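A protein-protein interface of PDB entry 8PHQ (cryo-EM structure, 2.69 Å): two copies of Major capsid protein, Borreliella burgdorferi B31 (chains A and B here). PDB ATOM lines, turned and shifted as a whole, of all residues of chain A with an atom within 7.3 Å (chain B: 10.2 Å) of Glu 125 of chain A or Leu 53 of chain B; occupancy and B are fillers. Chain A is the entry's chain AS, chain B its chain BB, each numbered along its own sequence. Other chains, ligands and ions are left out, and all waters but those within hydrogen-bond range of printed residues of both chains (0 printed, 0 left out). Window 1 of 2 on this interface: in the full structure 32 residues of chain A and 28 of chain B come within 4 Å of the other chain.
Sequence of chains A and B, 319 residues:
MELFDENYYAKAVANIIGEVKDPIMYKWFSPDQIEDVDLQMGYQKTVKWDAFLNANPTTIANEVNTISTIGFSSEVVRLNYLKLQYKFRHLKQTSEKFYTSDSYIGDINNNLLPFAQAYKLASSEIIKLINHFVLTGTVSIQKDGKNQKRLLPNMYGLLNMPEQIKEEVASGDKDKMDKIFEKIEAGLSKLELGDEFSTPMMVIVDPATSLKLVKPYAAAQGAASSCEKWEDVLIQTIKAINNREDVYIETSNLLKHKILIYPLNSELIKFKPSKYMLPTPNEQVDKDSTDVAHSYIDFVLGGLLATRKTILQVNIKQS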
ATOM      1  N   VAL A  20      -2.974  17.654 -31.178  1.00  0.00           N
ATOM      2  CA  VAL A  20      -3.566  16.603 -30.360  1.00  0.00           C
ATOM      3  C   VAL A  20      -4.746  15.986 -31.098  1.00  0.00           C
ATOM      4  O   VAL A  20      -5.575  16.692 -31.686  1.00  0.00           O
ATOM      5  CB  VAL A  20      -3.993  17.166 -28.995  1.00  0.00           C
ATOM      6  CG1 VAL A  20      -4.439  16.046 -28.074  1.00  0.00           C
ATOM      7  CG2 VAL A  20      -2.858  17.958 -28.370  1.00  0.00           C
ATOM      8  N   TYR A  86      -2.083  16.576 -13.222  1.00  0.00           N
ATOM      9  CA  TYR A  86      -0.811  15.900 -13.431  1.00  0.00           C
ATOM     10  C   TYR A  86       0.301  16.935 -13.533  1.00  0.00           C
ATOM     11  O   TYR A  86       0.060  18.104 -13.840  1.00  0.00           O
ATOM     12  CB  TYR A  86      -0.822  15.039 -14.700  1.00  0.00           C
ATOM     13  CG  TYR A  86      -1.217  13.598 -14.489  1.00  0.00           C
ATOM     14  CD1 TYR A  86      -0.445  12.755 -13.706  1.00  0.00           C
ATOM     15  CD2 TYR A  86      -2.354  13.075 -15.087  1.00  0.00           C
ATOM     16  CE1 TYR A  86      -0.797  11.436 -13.518  1.00  0.00           C
ATOM     17  CE2 TYR A  86      -2.714  11.759 -14.902  1.00  0.00           C
ATOM     18  CZ  TYR A  86      -1.933  10.943 -14.118  1.00  0.00           C
ATOM     19  OH  TYR A  86      -2.292   9.630 -13.933  1.00  0.00           O
ATOM     20  N   TYR A 119       4.025  18.820 -23.571  1.00  0.00           N
ATOM     21  CA  TYR A 119       2.609  19.078 -23.360  1.00  0.00           C
ATOM     22  C   TYR A 119       1.749  18.241 -24.292  1.00  0.00           C
ATOM     23  O   TYR A 119       0.736  17.677 -23.867  1.00  0.00           O
ATOM     24  CB  TYR A 119       2.315  20.562 -23.566  1.00  0.00           C
ATOM     25  CG  TYR A 119       0.858  20.910 -23.410  1.00  0.00           C
ATOM     26  CD1 TYR A 119       0.244  20.876 -22.167  1.00  0.00           C
ATOM     27  CD2 TYR A 119       0.085  21.239 -24.514  1.00  0.00           C
ATOM     28  CE1 TYR A 119      -1.091  21.184 -22.025  1.00  0.00           C
ATOM     29  CE2 TYR A 119      -1.250  21.546 -24.381  1.00  0.00           C
ATOM     30  CZ  TYR A 119      -1.834  21.517 -23.136  1.00  0.00           C
ATOM     31  OH  TYR A 119      -3.166  21.822 -23.000  1.00  0.00           O
ATOM     32  N   LYS A 120       2.131  18.152 -25.567  1.00  0.00           N
ATOM     33  CA  LYS A 120       1.341  17.375 -26.517  1.00  0.00           C
ATOM     34  C   LYS A 120       1.278  15.908 -26.107  1.00  0.00           C
ATOM     35  O   LYS A 120       0.199  15.299 -26.082  1.00  0.00           O
ATOM     36  CB  LYS A 120       1.928  17.519 -27.922  1.00  0.00           C
ATOM     37  CG  LYS A 120       1.040  16.975 -29.025  1.00  0.00           C
ATOM     38  CD  LYS A 120       1.851  16.233 -30.071  1.00  0.00           C
ATOM     39  CE  LYS A 120       3.016  17.070 -30.561  1.00  0.00           C
ATOM     40  NZ  LYS A 120       3.849  16.323 -31.538  1.00  0.00           N
ATOM     41  N   LEU A 121       2.429  15.330 -25.760  1.00  0.00           N
ATOM     42  CA  LEU A 121       2.455  13.916 -25.391  1.00  0.00           C
ATOM     43  C   LEU A 121       1.653  13.657 -24.117  1.00  0.00           C
ATOM     44  O   LEU A 121       0.873  12.690 -24.043  1.00  0.00           O
ATOM     45  CB  LEU A 121       3.902  13.456 -25.225  1.00  0.00           C
ATOM     46  CG  LEU A 121       4.759  13.472 -26.492  1.00  0.00           C
ATOM     47  CD1 LEU A 121       6.102  12.814 -26.237  1.00  0.00           C
ATOM     48  CD2 LEU A 121       4.038  12.796 -27.646  1.00  0.00           C
ATOM     49  N   ALA A 122       1.820  14.518 -23.109  1.00  0.00           N
ATOM     50  CA  ALA A 122       1.085  14.342 -21.862  1.00  0.00           C
ATOM     51  C   ALA A 122      -0.415  14.485 -22.081  1.00  0.00           C
ATOM     52  O   ALA A 122      -1.210  13.736 -21.498  1.00  0.00           O
ATOM     53  CB  ALA A 122       1.578  15.344 -20.821  1.00  0.00           C
ATOM     54  N   SER A 123      -0.823  15.441 -22.920  1.00  0.00           N
ATOM     55  CA  SER A 123      -2.238  15.607 -23.220  1.00  0.00           C
ATOM     56  C   SER A 123      -2.804  14.370 -23.895  1.00  0.00           C
ATOM     57  O   SER A 123      -3.928  13.955 -23.594  1.00  0.00           O
ATOM     58  CB  SER A 123      -2.450  16.840 -24.097  1.00  0.00           C
ATOM     59  OG  SER A 123      -2.025  18.016 -23.435  1.00  0.00           O
ATOM     60  N   SER A 124      -2.046  13.767 -24.815  1.00  0.00           N
ATOM     61  CA  SER A 124      -2.525  12.544 -25.456  1.00  0.00           C
ATOM     62  C   SER A 124      -2.738  11.428 -24.436  1.00  0.00           C
ATOM     63  O   SER A 124      -3.769  10.737 -24.460  1.00  0.00           O
ATOM     64  CB  SER A 124      -1.543  12.100 -26.539  1.00  0.00           C
ATOM     65  OG  SER A 124      -1.332  13.130 -27.487  1.00  0.00           O
ATOM     66  N   GLU A 125      -1.779  11.246 -23.524  1.00  0.00           N
ATOM     67  CA  GLU A 125      -1.936  10.207 -22.506  1.00  0.00           C
ATOM     68  C   GLU A 125      -3.148  10.474 -21.615  1.00  0.00           C
ATOM     69  O   GLU A 125      -3.920   9.555 -21.296  1.00  0.00           O
ATOM     70  CB  GLU A 125      -0.665  10.096 -21.663  1.00  0.00           C
ATOM     71  CG  GLU A 125       0.567   9.695 -22.450  1.00  0.00           C
ATOM     72  CD  GLU A 125       0.435   8.316 -23.063  1.00  0.00           C
ATOM     73  OE1 GLU A 125       0.290   7.339 -22.299  1.00  0.00           O
ATOM     74  OE2 GLU A 125       0.474   8.209 -24.305  1.00  0.00           O
ATOM     75  N   ILE A 126      -3.338  11.733 -21.214  1.00  0.00           N
ATOM     76  CA  ILE A 126      -4.466  12.072 -20.351  1.00  0.00           C
ATOM     77  C   ILE A 126      -5.785  11.841 -21.078  1.00  0.00           C
ATOM     78  O   ILE A 126      -6.770  11.391 -20.480  1.00  0.00           O
ATOM     79  CB  ILE A 126      -4.330  13.519 -19.845  1.00  0.00           C
ATOM     80  CG1 ILE A 126      -3.109  13.642 -18.933  1.00  0.00           C
ATOM     81  CG2 ILE A 126      -5.581  13.952 -19.103  1.00  0.00           C
ATOM     82  CD1 ILE A 126      -2.900  15.026 -18.372  1.00  0.00           C
ATOM     83  N   ILE A 127      -5.830  12.145 -22.378  1.00  0.00           N
ATOM     84  CA  ILE A 127      -7.042  11.905 -23.157  1.00  0.00           C
ATOM     85  C   ILE A 127      -7.362  10.417 -23.211  1.00  0.00           C
ATOM     86  O   ILE A 127      -8.530  10.016 -23.119  1.00  0.00           O
ATOM     87  CB  ILE A 127      -6.906  12.514 -24.565  1.00  0.00           C
ATOM     88  CG1 ILE A 127      -6.955  14.039 -24.486  1.00  0.00           C
ATOM     89  CG2 ILE A 127      -7.998  11.999 -25.483  1.00  0.00           C
ATOM     90  CD1 ILE A 127      -7.013  14.721 -25.831  1.00  0.00           C
ATOM     91  N   LYS A 128      -6.342   9.573 -23.371  1.00  0.00           N
ATOM     92  CA  LYS A 128      -6.601   8.132 -23.326  1.00  0.00           C
ATOM     93  C   LYS A 128      -7.160   7.711 -21.969  1.00  0.00           C
ATOM     94  O   LYS A 128      -8.071   6.872 -21.892  1.00  0.00           O
ATOM     95  CB  LYS A 128      -5.337   7.342 -23.657  1.00  0.00           C
ATOM     96  CG  LYS A 128      -4.752   7.655 -25.019  1.00  0.00           C
ATOM     97  CD  LYS A 128      -3.352   7.092 -25.160  1.00  0.00           C
ATOM     98  CE  LYS A 128      -2.747   7.465 -26.502  1.00  0.00           C
ATOM     99  NZ  LYS A 128      -1.345   6.985 -26.625  1.00  0.00           N
ATOM    100  N   LEU A 129      -6.636   8.289 -20.885  1.00  0.00           N
ATOM    101  CA  LEU A 129      -7.177   7.976 -19.562  1.00  0.00           C
ATOM    102  C   LEU A 129      -8.642   8.396 -19.444  1.00  0.00           C
ATOM    103  O   LEU A 129      -9.465   7.670 -18.866  1.00  0.00           O
ATOM    104  CB  LEU A 129      -6.338   8.648 -18.476  1.00  0.00           C
ATOM    105  CG  LEU A 129      -6.760   8.346 -17.038  1.00  0.00           C
ATOM    106  CD1 LEU A 129      -6.406   6.917 -16.671  1.00  0.00           C
ATOM    107  CD2 LEU A 129      -6.115   9.324 -16.072  1.00  0.00           C
ATOM    108  N   ILE A 130      -8.983   9.567 -19.985  1.00  0.00           N
ATOM    109  CA  ILE A 130     -10.367  10.037 -19.949  1.00  0.00           C
ATOM    110  C   ILE A 130     -11.274   9.105 -20.745  1.00  0.00           C
ATOM    111  O   ILE A 130     -12.405   8.817 -20.334  1.00  0.00           O
ATOM    112  CB  ILE A 130     -10.459  11.488 -20.455  1.00  0.00           C
ATOM    113  CG1 ILE A 130      -9.572  12.403 -19.612  1.00  0.00           C
ATOM    114  CG2 ILE A 130     -11.897  11.973 -20.440  1.00  0.00           C
ATOM    115  CD1 ILE A 130      -9.549  13.839 -20.080  1.00  0.00           C
ATOM    116  N   ASN A 131     -10.804   8.632 -21.900  1.00  0.00           N
ATOM    117  CA  ASN A 131     -11.591   7.671 -22.671  1.00  0.00           C
ATOM    118  C   ASN A 131     -11.839   6.401 -21.870  1.00  0.00           C
ATOM    119  O   ASN A 131     -12.950   5.851 -21.882  1.00  0.00           O
ATOM    120  CB  ASN A 131     -10.892   7.339 -23.987  1.00  0.00           C
ATOM    121  CG  ASN A 131     -10.744   8.539 -24.887  1.00  0.00           C
ATOM    122  OD1 ASN A 131     -11.291   9.605 -24.612  1.00  0.00           O
ATOM    123  ND2 ASN A 131      -9.997   8.376 -25.971  1.00  0.00           N
ATOM    124  N   SER A 140      -7.806   3.738 -13.736  1.00  0.00           N
ATOM    125  CA  SER A 140      -6.670   2.886 -13.430  1.00  0.00           C
ATOM    126  C   SER A 140      -5.649   3.002 -14.551  1.00  0.00           C
ATOM    127  O   SER A 140      -5.999   3.278 -15.700  1.00  0.00           O
ATOM    128  CB  SER A 140      -7.094   1.424 -13.251  1.00  0.00           C
ATOM    129  OG  SER A 140      -5.974   0.597 -12.995  1.00  0.00           O
ATOM    130  N   ILE A 141      -4.381   2.789 -14.204  1.00  0.00           N
ATOM    131  CA  ILE A 141      -3.293   2.810 -15.171  1.00  0.00           C
ATOM    132  C   ILE A 141      -2.663   1.435 -15.342  1.00  0.00           C
ATOM    133  O   ILE A 141      -1.616   1.314 -15.984  1.00  0.00           O
ATOM    134  CB  ILE A 141      -2.225   3.849 -14.797  1.00  0.00           C
ATOM    135  CG1 ILE A 141      -1.510   3.431 -13.513  1.00  0.00           C
ATOM    136  CG2 ILE A 141      -2.849   5.222 -14.640  1.00  0.00           C
ATOM    137  CD1 ILE A 141      -0.265   4.228 -13.232  1.00  0.00           C
ATOM    138  N   PRO A 279      -7.768  18.143 -21.367  1.00  0.00           N
ATOM    139  CA  PRO A 279      -6.596  18.710 -20.685  1.00  0.00           C
ATOM    140  C   PRO A 279      -6.432  20.202 -20.939  1.00  0.00           C
ATOM    141  O   PRO A 279      -6.606  20.688 -22.058  1.00  0.00           O
ATOM    142  CB  PRO A 279      -5.432  17.913 -21.279  1.00  0.00           C
ATOM    143  CG  PRO A 279      -6.032  16.601 -21.619  1.00  0.00           C
ATOM    144  CD  PRO A 279      -7.431  16.899 -22.082  1.00  0.00           C
ATOM    145  N   LYS B  48      11.971   8.580 -31.566  1.00  0.00           N
ATOM    146  CA  LYS B  48      10.543   8.605 -31.279  1.00  0.00           C
ATOM    147  C   LYS B  48      10.337   8.869 -29.795  1.00  0.00           C
ATOM    148  O   LYS B  48      10.896   8.161 -28.950  1.00  0.00           O
ATOM    149  CB  LYS B  48       9.873   7.291 -31.681  1.00  0.00           C
ATOM    150  CG  LYS B  48       8.382   7.265 -31.399  1.00  0.00           C
ATOM    151  CD  LYS B  48       7.791   5.890 -31.630  1.00  0.00           C
ATOM    152  CE  LYS B  48       6.292   5.894 -31.378  1.00  0.00           C
ATOM    153  NZ  LYS B  48       5.691   4.545 -31.566  1.00  0.00           N
ATOM    154  N   TRP B  49       9.532   9.879 -29.484  1.00  0.00           N
ATOM    155  CA  TRP B  49       9.307  10.314 -28.114  1.00  0.00           C
ATOM    156  C   TRP B  49       7.967   9.790 -27.616  1.00  0.00           C
ATOM    157  O   TRP B  49       6.985   9.761 -28.362  1.00  0.00           O
ATOM    158  CB  TRP B  49       9.340  11.840 -28.023  1.00  0.00           C
ATOM    159  CG  TRP B  49      10.721  12.412 -28.044  1.00  0.00           C
ATOM    160  CD1 TRP B  49      11.319  13.064 -29.081  1.00  0.00           C
ATOM    161  CD2 TRP B  49      11.680  12.390 -26.980  1.00  0.00           C
ATOM    162  NE1 TRP B  49      12.589  13.447 -28.732  1.00  0.00           N
ATOM    163  CE2 TRP B  49      12.836  13.045 -27.446  1.00  0.00           C
ATOM    164  CE3 TRP B  49      11.673  11.878 -25.680  1.00  0.00           C
ATOM    165  CZ2 TRP B  49      13.971  13.203 -26.659  1.00  0.00           C
ATOM    166  CZ3 TRP B  49      12.803  12.036 -24.900  1.00  0.00           C
ATOM    167  CH2 TRP B  49      13.936  12.693 -25.392  1.00  0.00           C
ATOM    168  N   ASP B  50       7.933   9.377 -26.351  1.00  0.00           N
ATOM    169  CA  ASP B  50       6.724   8.833 -25.750  1.00  0.00           C
ATOM    170  C   ASP B  50       6.547   9.404 -24.351  1.00  0.00           C
ATOM    171  O   ASP B  50       7.495   9.883 -23.726  1.00  0.00           O
ATOM    172  CB  ASP B  50       6.763   7.301 -25.686  1.00  0.00           C
ATOM    173  CG  ASP B  50       6.975   6.666 -27.044  1.00  0.00           C
ATOM    174  OD1 ASP B  50       6.108   6.844 -27.925  1.00  0.00           O
ATOM    175  OD2 ASP B  50       8.010   5.993 -27.232  1.00  0.00           O
ATOM    176  N   ALA B  51       5.309   9.347 -23.868  1.00  0.00           N
ATOM    177  CA  ALA B  51       4.965   9.773 -22.520  1.00  0.00           C
ATOM    178  C   ALA B  51       4.197   8.661 -21.824  1.00  0.00           C
ATOM    179  O   ALA B  51       3.513   7.862 -22.467  1.00  0.00           O
ATOM    180  CB  ALA B  51       4.131  11.056 -22.528  1.00  0.00           C
ATOM    181  N   PHE B  52       4.318   8.613 -20.500  1.00  0.00           N
ATOM    182  CA  PHE B  52       3.661   7.577 -19.720  1.00  0.00           C
ATOM    183  C   PHE B  52       3.237   8.143 -18.374  1.00  0.00           C
ATOM    184  O   PHE B  52       3.835   9.097 -17.868  1.00  0.00           O
ATOM    185  CB  PHE B  52       4.573   6.357 -19.536  1.00  0.00           C
ATOM    186  CG  PHE B  52       5.932   6.687 -18.983  1.00  0.00           C
ATOM    187  CD1 PHE B  52       6.117   6.887 -17.625  1.00  0.00           C
ATOM    188  CD2 PHE B  52       7.023   6.803 -19.824  1.00  0.00           C
ATOM    189  CE1 PHE B  52       7.364   7.189 -17.119  1.00  0.00           C
ATOM    190  CE2 PHE B  52       8.272   7.107 -19.323  1.00  0.00           C
ATOM    191  CZ  PHE B  52       8.442   7.300 -17.968  1.00  0.00           C
ATOM    192  N   LEU B  53       2.200   7.541 -17.800  1.00  0.00           N
ATOM    193  CA  LEU B  53       1.683   7.945 -16.501  1.00  0.00           C
ATOM    194  C   LEU B  53       2.354   7.123 -15.408  1.00  0.00           C
ATOM    195  O   LEU B  53       2.419   5.894 -15.501  1.00  0.00           O
ATOM    196  CB  LEU B  53       0.167   7.763 -16.448  1.00  0.00           C
ATOM    197  CG  LEU B  53      -0.636   8.379 -17.594  1.00  0.00           C
ATOM    198  CD1 LEU B  53      -2.121   8.119 -17.415  1.00  0.00           C
ATOM    199  CD2 LEU B  53      -0.366   9.867 -17.697  1.00  0.00           C
ATOM    200  N   ASN B  54       2.852   7.803 -14.377  1.00  0.00           N
ATOM    201  CA  ASN B  54       3.528   7.121 -13.279  1.00  0.00           C
ATOM    202  C   ASN B  54       2.574   6.631 -12.200  1.00  0.00           C
ATOM    203  O   ASN B  54       2.875   5.637 -11.530  1.00  0.00           O
ATOM    204  CB  ASN B  54       4.573   8.039 -12.642  1.00  0.00           C
ATOM    205  CG  ASN B  54       5.886   8.032 -13.391  1.00  0.00           C
ATOM    206  OD1 ASN B  54       6.531   6.994 -13.519  1.00  0.00           O
ATOM    207  ND2 ASN B  54       6.295   9.193 -13.882  1.00  0.00           N
ATOM    208  N   ALA B  55       1.441   7.298 -12.012  1.00  0.00           N
ATOM    209  CA  ALA B  55       0.498   6.920 -10.968  1.00  0.00           C
ATOM    210  C   ALA B  55      -0.876   7.460 -11.340  1.00  0.00           C
ATOM    211  O   ALA B  55      -1.057   8.083 -12.389  1.00  0.00           O
ATOM    212  CB  ALA B  55       0.953   7.436  -9.600  1.00  0.00           C
ATOM    213  N   ASN B  56      -1.847   7.208 -10.469  1.00  0.00           N
ATOM    214  CA  ASN B  56      -3.172   7.769 -10.654  1.00  0.00           C
ATOM    215  C   ASN B  56      -3.119   9.287 -10.497  1.00  0.00           C
ATOM    216  O   ASN B  56      -2.268   9.815  -9.779  1.00  0.00           O
ATOM    217  CB  ASN B  56      -4.153   7.177  -9.647  1.00  0.00           C
ATOM    218  CG  ASN B  56      -4.381   5.696  -9.857  1.00  0.00           C
ATOM    219  OD1 ASN B  56      -4.777   5.265 -10.937  1.00  0.00           O
ATOM    220  ND2 ASN B  56      -4.142   4.908  -8.817  1.00  0.00           N
ATOM    221  N   PRO B  57      -4.014  10.012 -11.166  1.00  0.00           N
ATOM    222  CA  PRO B  57      -4.011  11.472 -11.051  1.00  0.00           C
ATOM    223  C   PRO B  57      -4.311  11.922  -9.629  1.00  0.00           C
ATOM    224  O   PRO B  57      -4.778  11.155  -8.787  1.00  0.00           O
ATOM    225  CB  PRO B  57      -5.115  11.907 -12.024  1.00  0.00           C
ATOM    226  CG  PRO B  57      -5.971  10.696 -12.180  1.00  0.00           C
ATOM    227  CD  PRO B  57      -5.028   9.543 -12.123  1.00  0.00           C
ATOM    228  N   THR B  58      -4.022  13.192  -9.368  1.00  0.00           N
ATOM    229  CA  THR B  58      -4.156  13.773  -8.039  1.00  0.00           C
ATOM    230  C   THR B  58      -5.428  14.608  -7.965  1.00  0.00           C
ATOM    231  O   THR B  58      -5.701  15.409  -8.862  1.00  0.00           O
ATOM    232  CB  THR B  58      -2.938  14.636  -7.703  1.00  0.00           C
ATOM    233  OG1 THR B  58      -1.779  13.804  -7.590  1.00  0.00           O
ATOM    234  CG2 THR B  58      -3.146  15.380  -6.395  1.00  0.00           C
ATOM    235  N   SER B  68       1.047  13.743  -8.778  1.00  0.00           N
ATOM    236  CA  SER B  68       1.517  12.650  -9.618  1.00  0.00           C
ATOM    237  C   SER B  68       2.189  13.193 -10.874  1.00  0.00           C
ATOM    238  O   SER B  68       1.826  14.250 -11.393  1.00  0.00           O
ATOM    239  CB  SER B  68       0.361  11.730 -10.000  1.00  0.00           C
ATOM    240  OG  SER B  68      -0.150  11.056  -8.866  1.00  0.00           O
ATOM    241  N   THR B  69       3.174  12.449 -11.367  1.00  0.00           N
ATOM    242  CA  THR B  69       4.032  12.909 -12.446  1.00  0.00           C
ATOM    243  C   THR B  69       3.812  12.097 -13.715  1.00  0.00           C
ATOM    244  O   THR B  69       3.393  10.937 -13.671  1.00  0.00           O
ATOM    245  CB  THR B  69       5.508  12.833 -12.045  1.00  0.00           C
ATOM    246  OG1 THR B  69       5.850  11.478 -11.731  1.00  0.00           O
ATOM    247  CG2 THR B  69       5.777  13.712 -10.837  1.00  0.00           C
ATOM    248  N   ILE B  70       4.097  12.730 -14.850  1.00  0.00           N
ATOM    249  CA  ILE B  70       4.093  12.084 -16.158  1.00  0.00           C
ATOM    250  C   ILE B  70       5.527  12.055 -16.664  1.00  0.00           C
ATOM    251  O   ILE B  70       6.182  13.099 -16.754  1.00  0.00           O
ATOM    252  CB  ILE B  70       3.175  12.813 -17.152  1.00  0.00           C
ATOM    253  CG1 ILE B  70       1.724  12.771 -16.678  1.00  0.00           C
ATOM    254  CG2 ILE B  70       3.310  12.216 -18.541  1.00  0.00           C
ATOM    255  CD1 ILE B  70       0.775  13.515 -17.582  1.00  0.00           C
ATOM    256  N   GLY B  71       6.017  10.859 -16.991  1.00  0.00           N
ATOM    257  CA  GLY B  71       7.368  10.695 -17.478  1.00  0.00           C
ATOM    258  C   GLY B  71       7.454  10.728 -18.994  1.00  0.00           C
ATOM    259  O   GLY B  71       6.457  10.813 -19.708  1.00  0.00           O
ATOM    260  N   PHE B  72       8.689  10.660 -19.485  1.00  0.00           N
ATOM    261  CA  PHE B  72       8.961  10.677 -20.914  1.00  0.00           C
ATOM    262  C   PHE B  72      10.063   9.680 -21.232  1.00  0.00           C
ATOM    263  O   PHE B  72      10.948   9.426 -20.411  1.00  0.00           O
ATOM    264  CB  PHE B  72       9.360  12.077 -21.390  1.00  0.00           C
ATOM    265  CG  PHE B  72       8.274  13.097 -21.237  1.00  0.00           C
ATOM    266  CD1 PHE B  72       7.157  13.065 -22.051  1.00  0.00           C
ATOM    267  CD2 PHE B  72       8.356  14.076 -20.264  1.00  0.00           C
ATOM    268  CE1 PHE B  72       6.154  13.998 -21.909  1.00  0.00           C
ATOM    269  CE2 PHE B  72       7.354  15.010 -20.116  1.00  0.00           C
ATOM    270  CZ  PHE B  72       6.252  14.970 -20.938  1.00  0.00           C
ATOM    271  N   SER B  73      10.002   9.116 -22.436  1.00  0.00           N
ATOM    272  CA  SER B  73      10.972   8.128 -22.877  1.00  0.00           C
ATOM    273  C   SER B  73      11.247   8.322 -24.360  1.00  0.00           C
ATOM    274  O   SER B  73      10.418   8.853 -25.103  1.00  0.00           O
ATOM    275  CB  SER B  73      10.485   6.701 -22.607  1.00  0.00           C
ATOM    276  OG  SER B  73      11.452   5.750 -23.010  1.00  0.00           O
ATOM    277  N   ASP B 195      -3.383   0.017 -29.353  1.00  0.00           N
ATOM    278  CA  ASP B 195      -4.372   1.073 -29.530  1.00  0.00           C
ATOM    279  C   ASP B 195      -4.530   1.504 -30.981  1.00  0.00           C
ATOM    280  O   ASP B 195      -5.419   2.309 -31.279  1.00  0.00           O
ATOM    281  CB  ASP B 195      -4.001   2.286 -28.672  1.00  0.00           C
ATOM    282  CG  ASP B 195      -5.201   3.152 -28.330  1.00  0.00           C
ATOM    283  OD1 ASP B 195      -6.337   2.772 -28.686  1.00  0.00           O
ATOM    284  OD2 ASP B 195      -5.008   4.215 -27.707  1.00  0.00           O
ATOM    285  N   GLU B 196      -3.696   0.997 -31.887  1.00  0.00           N
ATOM    286  CA  GLU B 196      -3.742   1.368 -33.294  1.00  0.00           C
ATOM    287  C   GLU B 196      -4.433   0.313 -34.150  1.00  0.00           C
ATOM    288  O   GLU B 196      -4.241   0.293 -35.370  1.00  0.00           O
ATOM    289  CB  GLU B 196      -2.325   1.624 -33.811  1.00  0.00           C
ATOM    290  CG  GLU B 196      -1.579   2.725 -33.075  1.00  0.00           C
ATOM    291  CD  GLU B 196      -2.059   4.118 -33.439  1.00  0.00           C
ATOM    292  OE1 GLU B 196      -2.942   4.243 -34.314  1.00  0.00           O
ATOM    293  OE2 GLU B 196      -1.555   5.092 -32.845  1.00  0.00           O
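The side-chain carboxylate (OE1) of Glu 125 of chain A sits close to the backbone carbonyl oxygen (O) of Ala 51 of chain B.
OH of Tyr 86 of chain A is in hydrogen-bond range of O of Ala 55 of chain B (2.5 Å).
The side-chain hydroxyl (OH) of Tyr 86 of chain A lies close to the backbone nitrogen (N) of Pro 57 of chain B (3.3 Å).
The side-chain amide nitrogen (ND2) of Asn 54 of chain B sits at hydrogen-bond distance from the side-chain hydroxyl (OG1) of Thr 69 of chain B (3.2 Å).
N of Asp 50 of chain B sits at hydrogen-bond distance from O of Ser 73 of chain B, at 2.8 Å.
OG of Ser 68 of chain B lies within hydrogen-bond range of O of Asn 56 of chain B.
N of Ser 68 of chain B is in hydrogen-bond range of OG1 of Thr 58 of chain B, at 3.1 Å.
NZ of Lys 128 of chain A lies within salt-bridge range of OE2 of Glu 125 of chain A, at 3.2 Å.
Among the printed residues, merely in contact across the chains: Tyr 86 of chain A with Asn 56 of chain B, Tyr 86 of chain A with Ser 68 of chain B, Ile 141 of chain A with Ala 55 of chain B, Leu 121 of chain A with Ala 51 of chain B, Tyr 86 of chain A with Ile 70 of chain B, Tyr 86 of chain A with Leu 53 of chain B, Ala 122 of chain A with Ile 70 of chain B, Leu 121 of chain A with Trp 49 of chain B, Ile 141 of chain A with Asn 54 of chain B, Ile 141 of chain A with Leu 53 of chain B, Leu 121 of chain A with Asp 50 of chain B, Ser 140 of chain A with Asn 56 of chain B and Glu 125 of chain A with Leu 53 of chain B.
Of the printed residues of chain B, Glu 125 of chain A touches Ala 51 and Leu 53.
Ala 122 of chain A touches one residue of chain B.
No residue of chain B comes within 4 Å of Ser 124 of chain A.
No residue of chain B comes within 4 Å of Lys 128 of chain A.
Of the printed residues of chain A, Asp 50 of chain B touches Leu 121 (3.9 Å).
Of the printed residues of chain A, Pro 57 of chain B touches Tyr 86.
The nearest printed residue of chain B that does not touch Glu 125 of chain A is Phe 52 of chain B (4.3 Å).
Printed residues of chain A that touch a printed residue of chain B: Tyr 86, Leu 121, Ala 122, Glu 125, Ser 140 and Ile 141.
Hydrophobic or aromatic side chains of chain A that line the printed part of chain B: Tyr 86, Leu 121, Ala 122 and Ile 141.
Along chain A the printed residues that touch a printed residue of chain B span positions 86 to 141.
Of the 19 printed residues of chain B, 10 touch a printed residue of chain A.
Among the printed residues, no Asp or Glu carboxylate lies within 4 Å of a Lys or Arg side-chain nitrogen of the other chain.
No position is printed for both chains.
Of the 16 pairs that touch across the chains among the printed residues, none has its exchanged pair printed and touching as well.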
